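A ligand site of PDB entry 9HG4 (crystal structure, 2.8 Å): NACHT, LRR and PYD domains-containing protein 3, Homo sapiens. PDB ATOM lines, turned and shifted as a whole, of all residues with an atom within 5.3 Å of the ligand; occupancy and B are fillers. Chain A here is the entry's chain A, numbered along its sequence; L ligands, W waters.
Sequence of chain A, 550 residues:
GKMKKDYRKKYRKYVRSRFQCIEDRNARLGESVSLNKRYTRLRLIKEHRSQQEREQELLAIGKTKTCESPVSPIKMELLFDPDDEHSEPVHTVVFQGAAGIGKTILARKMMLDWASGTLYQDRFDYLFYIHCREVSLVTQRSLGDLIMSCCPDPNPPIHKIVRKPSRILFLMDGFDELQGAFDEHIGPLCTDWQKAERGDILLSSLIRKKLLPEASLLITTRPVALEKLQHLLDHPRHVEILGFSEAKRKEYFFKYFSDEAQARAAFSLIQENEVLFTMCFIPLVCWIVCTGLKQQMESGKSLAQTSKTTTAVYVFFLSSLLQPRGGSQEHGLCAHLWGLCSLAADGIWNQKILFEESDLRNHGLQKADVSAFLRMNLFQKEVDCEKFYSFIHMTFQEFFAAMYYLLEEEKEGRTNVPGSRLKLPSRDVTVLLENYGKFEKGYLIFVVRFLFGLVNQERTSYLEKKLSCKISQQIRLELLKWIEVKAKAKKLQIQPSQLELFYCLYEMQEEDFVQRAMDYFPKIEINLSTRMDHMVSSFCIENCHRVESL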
ATOM      1  N   ILE A  22       2.772  35.078  31.907  1.00  0.00           N
ATOM      2  CA  ILE A  22       1.788  34.164  31.343  1.00  0.00           C
ATOM      3  C   ILE A  22       0.393  34.522  31.921  1.00  0.00           C
ATOM      4  O   ILE A  22      -0.605  34.472  31.208  1.00  0.00           O
ATOM      5  CB  ILE A  22       2.235  32.706  31.704  1.00  0.00           C
ATOM      6  CG1 ILE A  22       3.159  32.118  30.633  1.00  0.00           C
ATOM      7  CG2 ILE A  22       1.071  31.744  32.052  1.00  0.00           C
ATOM      8  CD1 ILE A  22       3.808  30.774  30.988  1.00  0.00           C
ATOM      9  N   ARG A  38       9.209  30.286  31.870  1.00  0.00           N
ATOM     10  CA  ARG A  38       8.565  28.969  31.891  1.00  0.00           C
ATOM     11  C   ARG A  38       8.018  28.579  30.477  1.00  0.00           C
ATOM     12  O   ARG A  38       7.537  27.457  30.303  1.00  0.00           O
ATOM     13  CB  ARG A  38       7.425  28.911  32.937  1.00  0.00           C
ATOM     14  CG  ARG A  38       7.384  27.601  33.739  1.00  0.00           C
ATOM     15  CD  ARG A  38       5.979  27.022  33.845  1.00  0.00           C
ATOM     16  NE  ARG A  38       5.446  27.050  35.210  1.00  0.00           N
ATOM     17  CZ  ARG A  38       4.218  27.459  35.532  1.00  0.00           C
ATOM     18  NH1 ARG A  38       3.391  27.906  34.605  1.00  0.00           N
ATOM     19  NH2 ARG A  38       3.814  27.429  36.801  1.00  0.00           N
ATOM     20  N   TYR A  39       8.083  29.497  29.486  1.00  0.00           N
ATOM     21  CA  TYR A  39       7.622  29.244  28.133  1.00  0.00           C
ATOM     22  C   TYR A  39       8.460  28.121  27.528  1.00  0.00           C
ATOM     23  O   TYR A  39       9.685  28.161  27.597  1.00  0.00           O
ATOM     24  CB  TYR A  39       7.703  30.519  27.258  1.00  0.00           C
ATOM     25  CG  TYR A  39       7.463  30.262  25.792  1.00  0.00           C
ATOM     26  CD1 TYR A  39       6.181  30.215  25.276  1.00  0.00           C
ATOM     27  CD2 TYR A  39       8.518  29.994  24.928  1.00  0.00           C
ATOM     28  CE1 TYR A  39       5.944  29.906  23.935  1.00  0.00           C
ATOM     29  CE2 TYR A  39       8.297  29.690  23.583  1.00  0.00           C
ATOM     30  CZ  TYR A  39       7.004  29.641  23.095  1.00  0.00           C
ATOM     31  OH  TYR A  39       6.764  29.340  21.775  1.00  0.00           O
ATOM     32  N   THR A  40       7.798  27.124  26.957  1.00  0.00           N
ATOM     33  CA  THR A  40       8.485  26.021  26.310  1.00  0.00           C
ATOM     34  C   THR A  40       8.087  26.046  24.838  1.00  0.00           C
ATOM     35  O   THR A  40       6.925  26.269  24.521  1.00  0.00           O
ATOM     36  CB  THR A  40       8.165  24.685  27.031  1.00  0.00           C
ATOM     37  OG1 THR A  40       8.665  24.725  28.363  1.00  0.00           O
ATOM     38  CG2 THR A  40       8.753  23.492  26.332  1.00  0.00           C
ATOM     39  N   ARG A  41       9.042  25.862  23.944  1.00  0.00           N
ATOM     40  CA  ARG A  41       8.794  25.934  22.518  1.00  0.00           C
ATOM     41  C   ARG A  41       7.655  25.024  22.038  1.00  0.00           C
ATOM     42  O   ARG A  41       7.619  23.853  22.362  1.00  0.00           O
ATOM     43  CB  ARG A  41      10.075  25.674  21.726  1.00  0.00           C
ATOM     44  CG  ARG A  41       9.979  26.097  20.272  1.00  0.00           C
ATOM     45  CD  ARG A  41      11.055  25.434  19.442  1.00  0.00           C
ATOM     46  NE  ARG A  41      12.347  26.110  19.621  1.00  0.00           N
ATOM     47  CZ  ARG A  41      13.529  25.515  19.473  1.00  0.00           C
ATOM     48  NH1 ARG A  41      13.596  24.210  19.196  1.00  0.00           N
ATOM     49  NH2 ARG A  41      14.647  26.204  19.633  1.00  0.00           N
ATOM     50  N   LEU A  42       6.711  25.591  21.302  1.00  0.00           N
ATOM     51  CA  LEU A  42       5.590  24.848  20.743  1.00  0.00           C
ATOM     52  C   LEU A  42       5.906  24.463  19.308  1.00  0.00           C
ATOM     53  O   LEU A  42       6.572  25.209  18.607  1.00  0.00           O
ATOM     54  CB  LEU A  42       4.317  25.697  20.780  1.00  0.00           C
ATOM     55  CG  LEU A  42       3.824  26.085  22.152  1.00  0.00           C
ATOM     56  CD1 LEU A  42       2.852  27.219  22.071  1.00  0.00           C
ATOM     57  CD2 LEU A  42       3.213  24.915  22.844  1.00  0.00           C
ATOM     58  N   GLY A  97      -5.415  25.516  16.777  1.00  0.00           N
ATOM     59  CA  GLY A  97      -4.851  24.724  17.863  1.00  0.00           C
ATOM     60  C   GLY A  97      -5.909  24.239  18.813  1.00  0.00           C
ATOM     61  O   GLY A  97      -6.845  24.975  19.145  1.00  0.00           O
ATOM     62  N   ALA A  98      -5.755  23.016  19.297  1.00  0.00           N
ATOM     63  CA  ALA A  98      -6.708  22.440  20.247  1.00  0.00           C
ATOM     64  C   ALA A  98      -6.814  23.278  21.533  1.00  0.00           C
ATOM     65  O   ALA A  98      -5.909  24.052  21.834  1.00  0.00           O
ATOM     66  CB  ALA A  98      -6.280  21.018  20.582  1.00  0.00           C
ATOM     67  N   ALA A  99      -7.905  23.124  22.312  1.00  0.00           N
ATOM     68  CA  ALA A  99      -8.050  23.865  23.566  1.00  0.00           C
ATOM     69  C   ALA A  99      -6.917  23.489  24.522  1.00  0.00           C
ATOM     70  O   ALA A  99      -6.558  22.313  24.593  1.00  0.00           O
ATOM     71  CB  ALA A  99      -9.402  23.590  24.202  1.00  0.00           C
ATOM     72  N   GLY A 100      -6.282  24.485  25.105  1.00  0.00           N
ATOM     73  CA  GLY A 100      -5.147  24.269  25.987  1.00  0.00           C
ATOM     74  C   GLY A 100      -3.814  24.032  25.288  1.00  0.00           C
ATOM     75  O   GLY A 100      -2.814  23.811  25.962  1.00  0.00           O
ATOM     76  N   ILE A 101      -3.782  24.086  23.941  1.00  0.00           N
ATOM     77  CA  ILE A 101      -2.528  23.872  23.195  1.00  0.00           C
ATOM     78  C   ILE A 101      -1.510  25.001  23.380  1.00  0.00           C
ATOM     79  O   ILE A 101      -0.331  24.794  23.097  1.00  0.00           O
ATOM     80  CB  ILE A 101      -2.761  23.555  21.685  1.00  0.00           C
ATOM     81  CG1 ILE A 101      -1.726  22.556  21.137  1.00  0.00           C
ATOM     82  CG2 ILE A 101      -2.797  24.812  20.820  1.00  0.00           C
ATOM     83  CD1 ILE A 101      -1.888  21.187  21.647  1.00  0.00           C
ATOM     84  N   GLY A 102      -1.963  26.186  23.798  1.00  0.00           N
ATOM     85  CA  GLY A 102      -1.058  27.306  23.995  1.00  0.00           C
ATOM     86  C   GLY A 102      -1.231  28.449  23.010  1.00  0.00           C
ATOM     87  O   GLY A 102      -0.265  29.159  22.733  1.00  0.00           O
ATOM     88  N   LYS A 103      -2.449  28.656  22.480  1.00  0.00           N
ATOM     89  CA  LYS A 103      -2.735  29.748  21.547  1.00  0.00           C
ATOM     90  C   LYS A 103      -2.498  31.106  22.234  1.00  0.00           C
ATOM     91  O   LYS A 103      -1.804  31.952  21.678  1.00  0.00           O
ATOM     92  CB  LYS A 103      -4.164  29.648  21.006  1.00  0.00           C
ATOM     93  CG  LYS A 103      -4.370  28.480  20.055  1.00  0.00           C
ATOM     94  CD  LYS A 103      -5.808  28.372  19.564  1.00  0.00           C
ATOM     95  CE  LYS A 103      -6.778  28.136  20.670  1.00  0.00           C
ATOM     96  NZ  LYS A 103      -6.584  26.824  21.321  1.00  0.00           N
ATOM     97  N   THR A 104      -3.011  31.290  23.457  1.00  0.00           N
ATOM     98  CA  THR A 104      -2.835  32.526  24.210  1.00  0.00           C
ATOM     99  C   THR A 104      -1.390  32.749  24.573  1.00  0.00           C
ATOM    100  O   THR A 104      -0.889  33.850  24.401  1.00  0.00           O
ATOM    101  CB  THR A 104      -3.725  32.558  25.457  1.00  0.00           C
ATOM    102  OG1 THR A 104      -5.081  32.597  25.049  1.00  0.00           O
ATOM    103  CG2 THR A 104      -3.439  33.750  26.343  1.00  0.00           C
ATOM    104  N   ILE A 105      -0.694  31.721  25.062  1.00  0.00           N
ATOM    105  CA  ILE A 105       0.710  31.848  25.436  1.00  0.00           C
ATOM    106  C   ILE A 105       1.559  32.199  24.199  1.00  0.00           C
ATOM    107  O   ILE A 105       2.424  33.060  24.290  1.00  0.00           O
ATOM    108  CB  ILE A 105       1.200  30.576  26.175  1.00  0.00           C
ATOM    109  CG1 ILE A 105       0.367  30.330  27.457  1.00  0.00           C
ATOM    110  CG2 ILE A 105       2.707  30.613  26.452  1.00  0.00           C
ATOM    111  CD1 ILE A 105       0.305  31.435  28.414  1.00  0.00           C
ATOM    112  N   LEU A 106       1.243  31.618  23.035  1.00  0.00           N
ATOM    113  CA  LEU A 106       1.963  31.933  21.814  1.00  0.00           C
ATOM    114  C   LEU A 106       1.700  33.361  21.379  1.00  0.00           C
ATOM    115  O   LEU A 106       2.641  34.071  20.998  1.00  0.00           O
ATOM    116  CB  LEU A 106       1.614  30.960  20.676  1.00  0.00           C
ATOM    117  CG  LEU A 106       2.499  31.025  19.454  1.00  0.00           C
ATOM    118  CD1 LEU A 106       4.006  30.917  19.827  1.00  0.00           C
ATOM    119  CD2 LEU A 106       2.138  29.938  18.496  1.00  0.00           C
ATOM    120  N   ASP A 173      -6.629  37.025  19.352  1.00  0.00           N
ATOM    121  CA  ASP A 173      -6.453  35.804  20.131  1.00  0.00           C
ATOM    122  C   ASP A 173      -7.745  35.167  20.625  1.00  0.00           C
ATOM    123  O   ASP A 173      -8.415  35.705  21.518  1.00  0.00           O
ATOM    124  CB  ASP A 173      -5.501  36.037  21.308  1.00  0.00           C
ATOM    125  CG  ASP A 173      -5.214  34.782  22.124  1.00  0.00           C
ATOM    126  OD1 ASP A 173      -5.252  33.671  21.536  1.00  0.00           O
ATOM    127  OD2 ASP A 173      -4.952  34.919  23.335  1.00  0.00           O
ATOM    128  N   GLU A 177     -13.660  32.182  21.124  1.00  0.00           N
ATOM    129  CA  GLU A 177     -14.075  32.742  22.418  1.00  0.00           C
ATOM    130  C   GLU A 177     -14.865  34.044  22.329  1.00  0.00           C
ATOM    131  O   GLU A 177     -15.074  34.697  23.352  1.00  0.00           O
ATOM    132  CB  GLU A 177     -12.881  32.925  23.348  1.00  0.00           C
ATOM    133  CG  GLU A 177     -12.217  31.617  23.711  1.00  0.00           C
ATOM    134  CD  GLU A 177     -11.074  31.733  24.693  1.00  0.00           C
ATOM    135  OE1 GLU A 177     -10.584  32.868  24.935  1.00  0.00           O
ATOM    136  OE2 GLU A 177     -10.652  30.681  25.232  1.00  0.00           O
ATOM    137  N   PHE A 244       3.379  20.353  22.543  1.00  0.00           N
ATOM    138  CA  PHE A 244       4.677  19.899  22.978  1.00  0.00           C
ATOM    139  C   PHE A 244       5.133  18.619  22.331  1.00  0.00           C
ATOM    140  O   PHE A 244       4.387  17.650  22.243  1.00  0.00           O
ATOM    141  CB  PHE A 244       4.704  19.703  24.496  1.00  0.00           C
ATOM    142  CG  PHE A 244       4.710  20.960  25.339  1.00  0.00           C
ATOM    143  CD1 PHE A 244       5.164  22.160  24.816  1.00  0.00           C
ATOM    144  CD2 PHE A 244       4.293  20.936  26.657  1.00  0.00           C
ATOM    145  CE1 PHE A 244       5.152  23.308  25.581  1.00  0.00           C
ATOM    146  CE2 PHE A 244       4.322  22.077  27.426  1.00  0.00           C
ATOM    147  CZ  PHE A 244       4.748  23.258  26.891  1.00  0.00           C
ATOM    148  N   TYR A 252       9.349  20.841  29.837  1.00  0.00           N
ATOM    149  CA  TYR A 252       8.340  21.475  30.667  1.00  0.00           C
ATOM    150  C   TYR A 252       8.408  20.989  32.107  1.00  0.00           C
ATOM    151  O   TYR A 252       8.454  21.814  33.009  1.00  0.00           O
ATOM    152  CB  TYR A 252       6.917  21.264  30.111  1.00  0.00           C
ATOM    153  CG  TYR A 252       5.879  22.001  30.938  1.00  0.00           C
ATOM    154  CD1 TYR A 252       5.308  21.409  32.056  1.00  0.00           C
ATOM    155  CD2 TYR A 252       5.544  23.315  30.651  1.00  0.00           C
ATOM    156  CE1 TYR A 252       4.422  22.107  32.860  1.00  0.00           C
ATOM    157  CE2 TYR A 252       4.628  24.009  31.433  1.00  0.00           C
ATOM    158  CZ  TYR A 252       4.073  23.400  32.546  1.00  0.00           C
ATOM    159  OH  TYR A 252       3.181  24.086  33.315  1.00  0.00           O
ATOM    160  N   PRO A 283      -0.004  21.516  26.443  1.00  0.00           N
ATOM    161  CA  PRO A 283       0.655  22.199  27.577  1.00  0.00           C
ATOM    162  C   PRO A 283      -0.237  22.439  28.795  1.00  0.00           C
ATOM    163  O   PRO A 283       0.262  22.414  29.920  1.00  0.00           O
ATOM    164  CB  PRO A 283       1.127  23.512  26.962  1.00  0.00           C
ATOM    165  CG  PRO A 283       1.259  23.220  25.520  1.00  0.00           C
ATOM    166  CD  PRO A 283       0.122  22.283  25.209  1.00  0.00           C
ATOM    167  N   LEU A 284      -1.553  22.592  28.589  1.00  0.00           N
ATOM    168  CA  LEU A 284      -2.482  22.747  29.714  1.00  0.00           C
ATOM    169  C   LEU A 284      -2.498  21.438  30.515  1.00  0.00           C
ATOM    170  O   LEU A 284      -2.457  21.491  31.736  1.00  0.00           O
ATOM    171  CB  LEU A 284      -3.891  23.114  29.234  1.00  0.00           C
ATOM    172  CG  LEU A 284      -4.967  23.155  30.309  1.00  0.00           C
ATOM    173  CD1 LEU A 284      -4.689  24.195  31.341  1.00  0.00           C
ATOM    174  CD2 LEU A 284      -6.326  23.361  29.707  1.00  0.00           C
ATOM    175  N   TRP A 287       0.548  21.306  32.662  1.00  0.00           N
ATOM    176  CA  TRP A 287       0.343  22.148  33.827  1.00  0.00           C
ATOM    177  C   TRP A 287      -0.580  21.475  34.856  1.00  0.00           C
ATOM    178  O   TRP A 287      -0.249  21.455  36.038  1.00  0.00           O
ATOM    179  CB  TRP A 287      -0.199  23.534  33.428  1.00  0.00           C
ATOM    180  CG  TRP A 287      -0.389  24.435  34.602  1.00  0.00           C
ATOM    181  CD1 TRP A 287       0.566  25.178  35.239  1.00  0.00           C
ATOM    182  CD2 TRP A 287      -1.612  24.651  35.328  1.00  0.00           C
ATOM    183  NE1 TRP A 287       0.003  25.853  36.307  1.00  0.00           N
ATOM    184  CE2 TRP A 287      -1.327  25.538  36.384  1.00  0.00           C
ATOM    185  CE3 TRP A 287      -2.920  24.160  35.198  1.00  0.00           C
ATOM    186  CZ2 TRP A 287      -2.294  25.958  37.289  1.00  0.00           C
ATOM    187  CZ3 TRP A 287      -3.881  24.596  36.075  1.00  0.00           C
ATOM    188  CH2 TRP A 287      -3.574  25.489  37.108  1.00  0.00           C
ATOM    189  N   HIS A 393      -9.115  28.139  32.925  1.00  0.00           N
ATOM    190  CA  HIS A 393      -9.195  27.775  31.520  1.00  0.00           C
ATOM    191  C   HIS A 393     -10.651  27.461  31.189  1.00  0.00           C
ATOM    192  O   HIS A 393     -11.415  27.043  32.058  1.00  0.00           O
ATOM    193  CB  HIS A 393      -8.268  26.607  31.145  1.00  0.00           C
ATOM    194  CG  HIS A 393      -8.079  26.445  29.659  1.00  0.00           C
ATOM    195  ND1 HIS A 393      -8.920  25.631  28.919  1.00  0.00           N
ATOM    196  CD2 HIS A 393      -7.174  27.004  28.829  1.00  0.00           C
ATOM    197  CE1 HIS A 393      -8.488  25.710  27.674  1.00  0.00           C
ATOM    198  NE2 HIS A 393      -7.449  26.529  27.559  1.00  0.00           N
ATOM    199  N   MET A 394     -11.043  27.689  29.946  1.00  0.00           N
ATOM    200  CA  MET A 394     -12.411  27.428  29.502  1.00  0.00           C
ATOM    201  C   MET A 394     -12.803  25.954  29.688  1.00  0.00           C
ATOM    202  O   MET A 394     -13.973  25.660  29.951  1.00  0.00           O
ATOM    203  CB  MET A 394     -12.622  27.879  28.052  1.00  0.00           C
ATOM    204  CG  MET A 394     -11.607  27.301  27.110  1.00  0.00           C
ATOM    205  SD  MET A 394     -12.290  26.551  25.622  1.00  0.00           S
ATOM    206  CE  MET A 394     -12.867  25.023  26.260  1.00  0.00           C
HETATM  207  P1  LIG L   1      -5.397  27.931  24.557  1.00  0.00           P
HETATM  208  O1  LIG L   1      -4.938  27.036  23.427  1.00  0.00           O
HETATM  209  O2  LIG L   1      -6.815  27.645  25.020  1.00  0.00           O
HETATM  210  O3  LIG L   1      -5.163  29.406  24.283  1.00  0.00           O
HETATM  211  P2  LIG L   1      -3.428  28.694  26.603  1.00  0.00           P
HETATM  212  O4  LIG L   1      -2.475  29.332  25.678  1.00  0.00           O
HETATM  213  O5  LIG L   1      -4.294  29.537  27.467  1.00  0.00           O
HETATM  214  O6  LIG L   1      -4.366  27.713  25.753  1.00  0.00           O
HETATM  215  O7  LIG L   1      -2.586  27.689  27.508  1.00  0.00           O
HETATM  216  C1  LIG L   1      -3.203  27.107  28.674  1.00  0.00           C
HETATM  217  C2  LIG L   1      -2.125  26.850  29.703  1.00  0.00           C
HETATM  218  O8  LIG L   1      -1.114  25.991  29.124  1.00  0.00           O
HETATM  219  C3  LIG L   1      -1.360  28.092  30.125  1.00  0.00           C
HETATM  220  O9  LIG L   1      -2.038  28.764  31.183  1.00  0.00           O
HETATM  221  C4  LIG L   1      -0.019  27.504  30.577  1.00  0.00           C
HETATM  222  O10 LIG L   1      -0.134  26.908  31.869  1.00  0.00           O
HETATM  223  C5  LIG L   1       0.176  26.374  29.570  1.00  0.00           C
HETATM  224  N1  LIG L   1       0.981  26.707  28.402  1.00  0.00           N
HETATM  225  C6  LIG L   1       0.541  26.810  27.112  1.00  0.00           C
HETATM  226  N2  LIG L   1       1.502  26.966  26.232  1.00  0.00           N
HETATM  227  C7  LIG L   1       2.657  26.969  26.998  1.00  0.00           C
HETATM  228  C8  LIG L   1       4.017  27.062  26.662  1.00  0.00           C
HETATM  229  N3  LIG L   1       4.459  27.204  25.414  1.00  0.00           N
HETATM  230  N4  LIG L   1       4.922  26.998  27.663  1.00  0.00           N
HETATM  231  C9  LIG L   1       4.473  26.847  28.918  1.00  0.00           C
HETATM  232  N5  LIG L   1       3.219  26.751  29.356  1.00  0.00           N
HETATM  233  C10 LIG L   1       2.350  26.812  28.346  1.00  0.00           C
HETATM  234  O   HOH W   1      -8.993  27.385  23.327  1.00  0.00           O
HETATM  235  O   HOH W   2      -2.549  28.075  33.764  1.00  0.00           O
HETATM  236  O   HOH W   3      -7.042  31.612  23.278  1.00  0.00           O
HETATM  237  O   HOH W   4       2.700  26.557  32.127  1.00  0.00           O
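Residues that only touch the ligand: Pro 283 (3.4 Å), Arg 38 (3.4 Å), Tyr 39 (3.4 Å), Leu 42 (3.5 Å), Ala 98 (3.5 Å), Trp 287 (3.7 Å), Tyr 252 (3.7 Å) and Phe 244 (3.8 Å). Hydrophobic or aromatic side chains within 4 Å of the ligand: Tyr 39, Leu 42, Ile 105, Phe 244, Tyr 252, Pro 283, Trp 287 and His 393. Within 4 Å of the ligand: Arg 38, Tyr 39, Thr 40, Leu 42, Ala 98, Gly 100, Ile 101, Gly 102, Lys 103, Thr 104, Ile 105, Phe 244, Tyr 252, Pro 283, Leu 284, Trp 287 and His 393.
Water W1 bridges O2 of the ligand (2.8 Å) and NZ of Lys 103 (3.2 Å). Water W4 lies within hydrogen-bond range of OH of Tyr 252 (2.8 Å), N5 of the ligand (2.8 Å) and NH1 of Arg 38 (2.9 Å). Water W3 lies within hydrogen-bond range of the side-chain hydroxyl of Thr 104 (2.8 Å), an oxygen (O3) of the ligand (3.1 Å) and the side-chain carboxylate of Asp 173 (3.2 Å).
An oxygen (O1) of the ligand lies within salt-bridge range of the side-chain amino group (NZ) of Lys 103 (2.7 Å). O2 of the ligand is in hydrogen-bond range of N of Gly 100. The backbone carbonyl oxygen (O) of Thr 40 lies within hydrogen-bond range of a nitrogen (N3) of the ligand, at 2.8 Å. A ring nitrogen (NE2) of His 393 lies within hydrogen-bond range of an oxygen (O2) of the ligand (2.8 Å). N of Lys 103 sits at hydrogen-bond distance from O1 of the ligand, at 3.1 Å. An oxygen (O4) of the ligand sits at hydrogen-bond distance from the backbone NH (N) of Ile 105 (3.0 Å). O8 of the ligand sits at hydrogen-bond distance from N of Leu 284 (3.5 Å). The backbone NH of Gly 102 is in hydrogen-bond range of an oxygen (O1) of the ligand (3.1 Å). A nitrogen (N4) of the ligand is in hydrogen-bond range of the backbone NH (N) of Thr 40 (3.0 Å). N of Thr 104 lies within hydrogen-bond range of O3 of the ligand (3.0 Å). An oxygen (O1) of the ligand sits at hydrogen-bond distance from the backbone NH of Ile 101 (3.2 Å). An oxygen (O3) of the ligand sits at hydrogen-bond distance from the side-chain hydroxyl (OG1) of Thr 104 (3.3 Å).
The side-chain hydroxyl (OG1) of Thr 104 sits at hydrogen-bond distance from the side-chain carboxylate (OD2) of Asp 173, at 2.9 Å. NZ of Lys 103 is in hydrogen-bond range of O of Ala 98 (2.9 Å). The backbone NH (N) of Gly 100 lies within hydrogen-bond range of a ring nitrogen (NE2) of His 393. The backbone carbonyl oxygen (O) of Gly 100 is in hydrogen-bond range of the backbone NH (N) of Leu 284, at 3.2 Å. The side-chain amino group (NZ) of Lys 103 lies within hydrogen-bond range of the backbone carbonyl oxygen (O) of Gly 97, 2.9 Å away.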
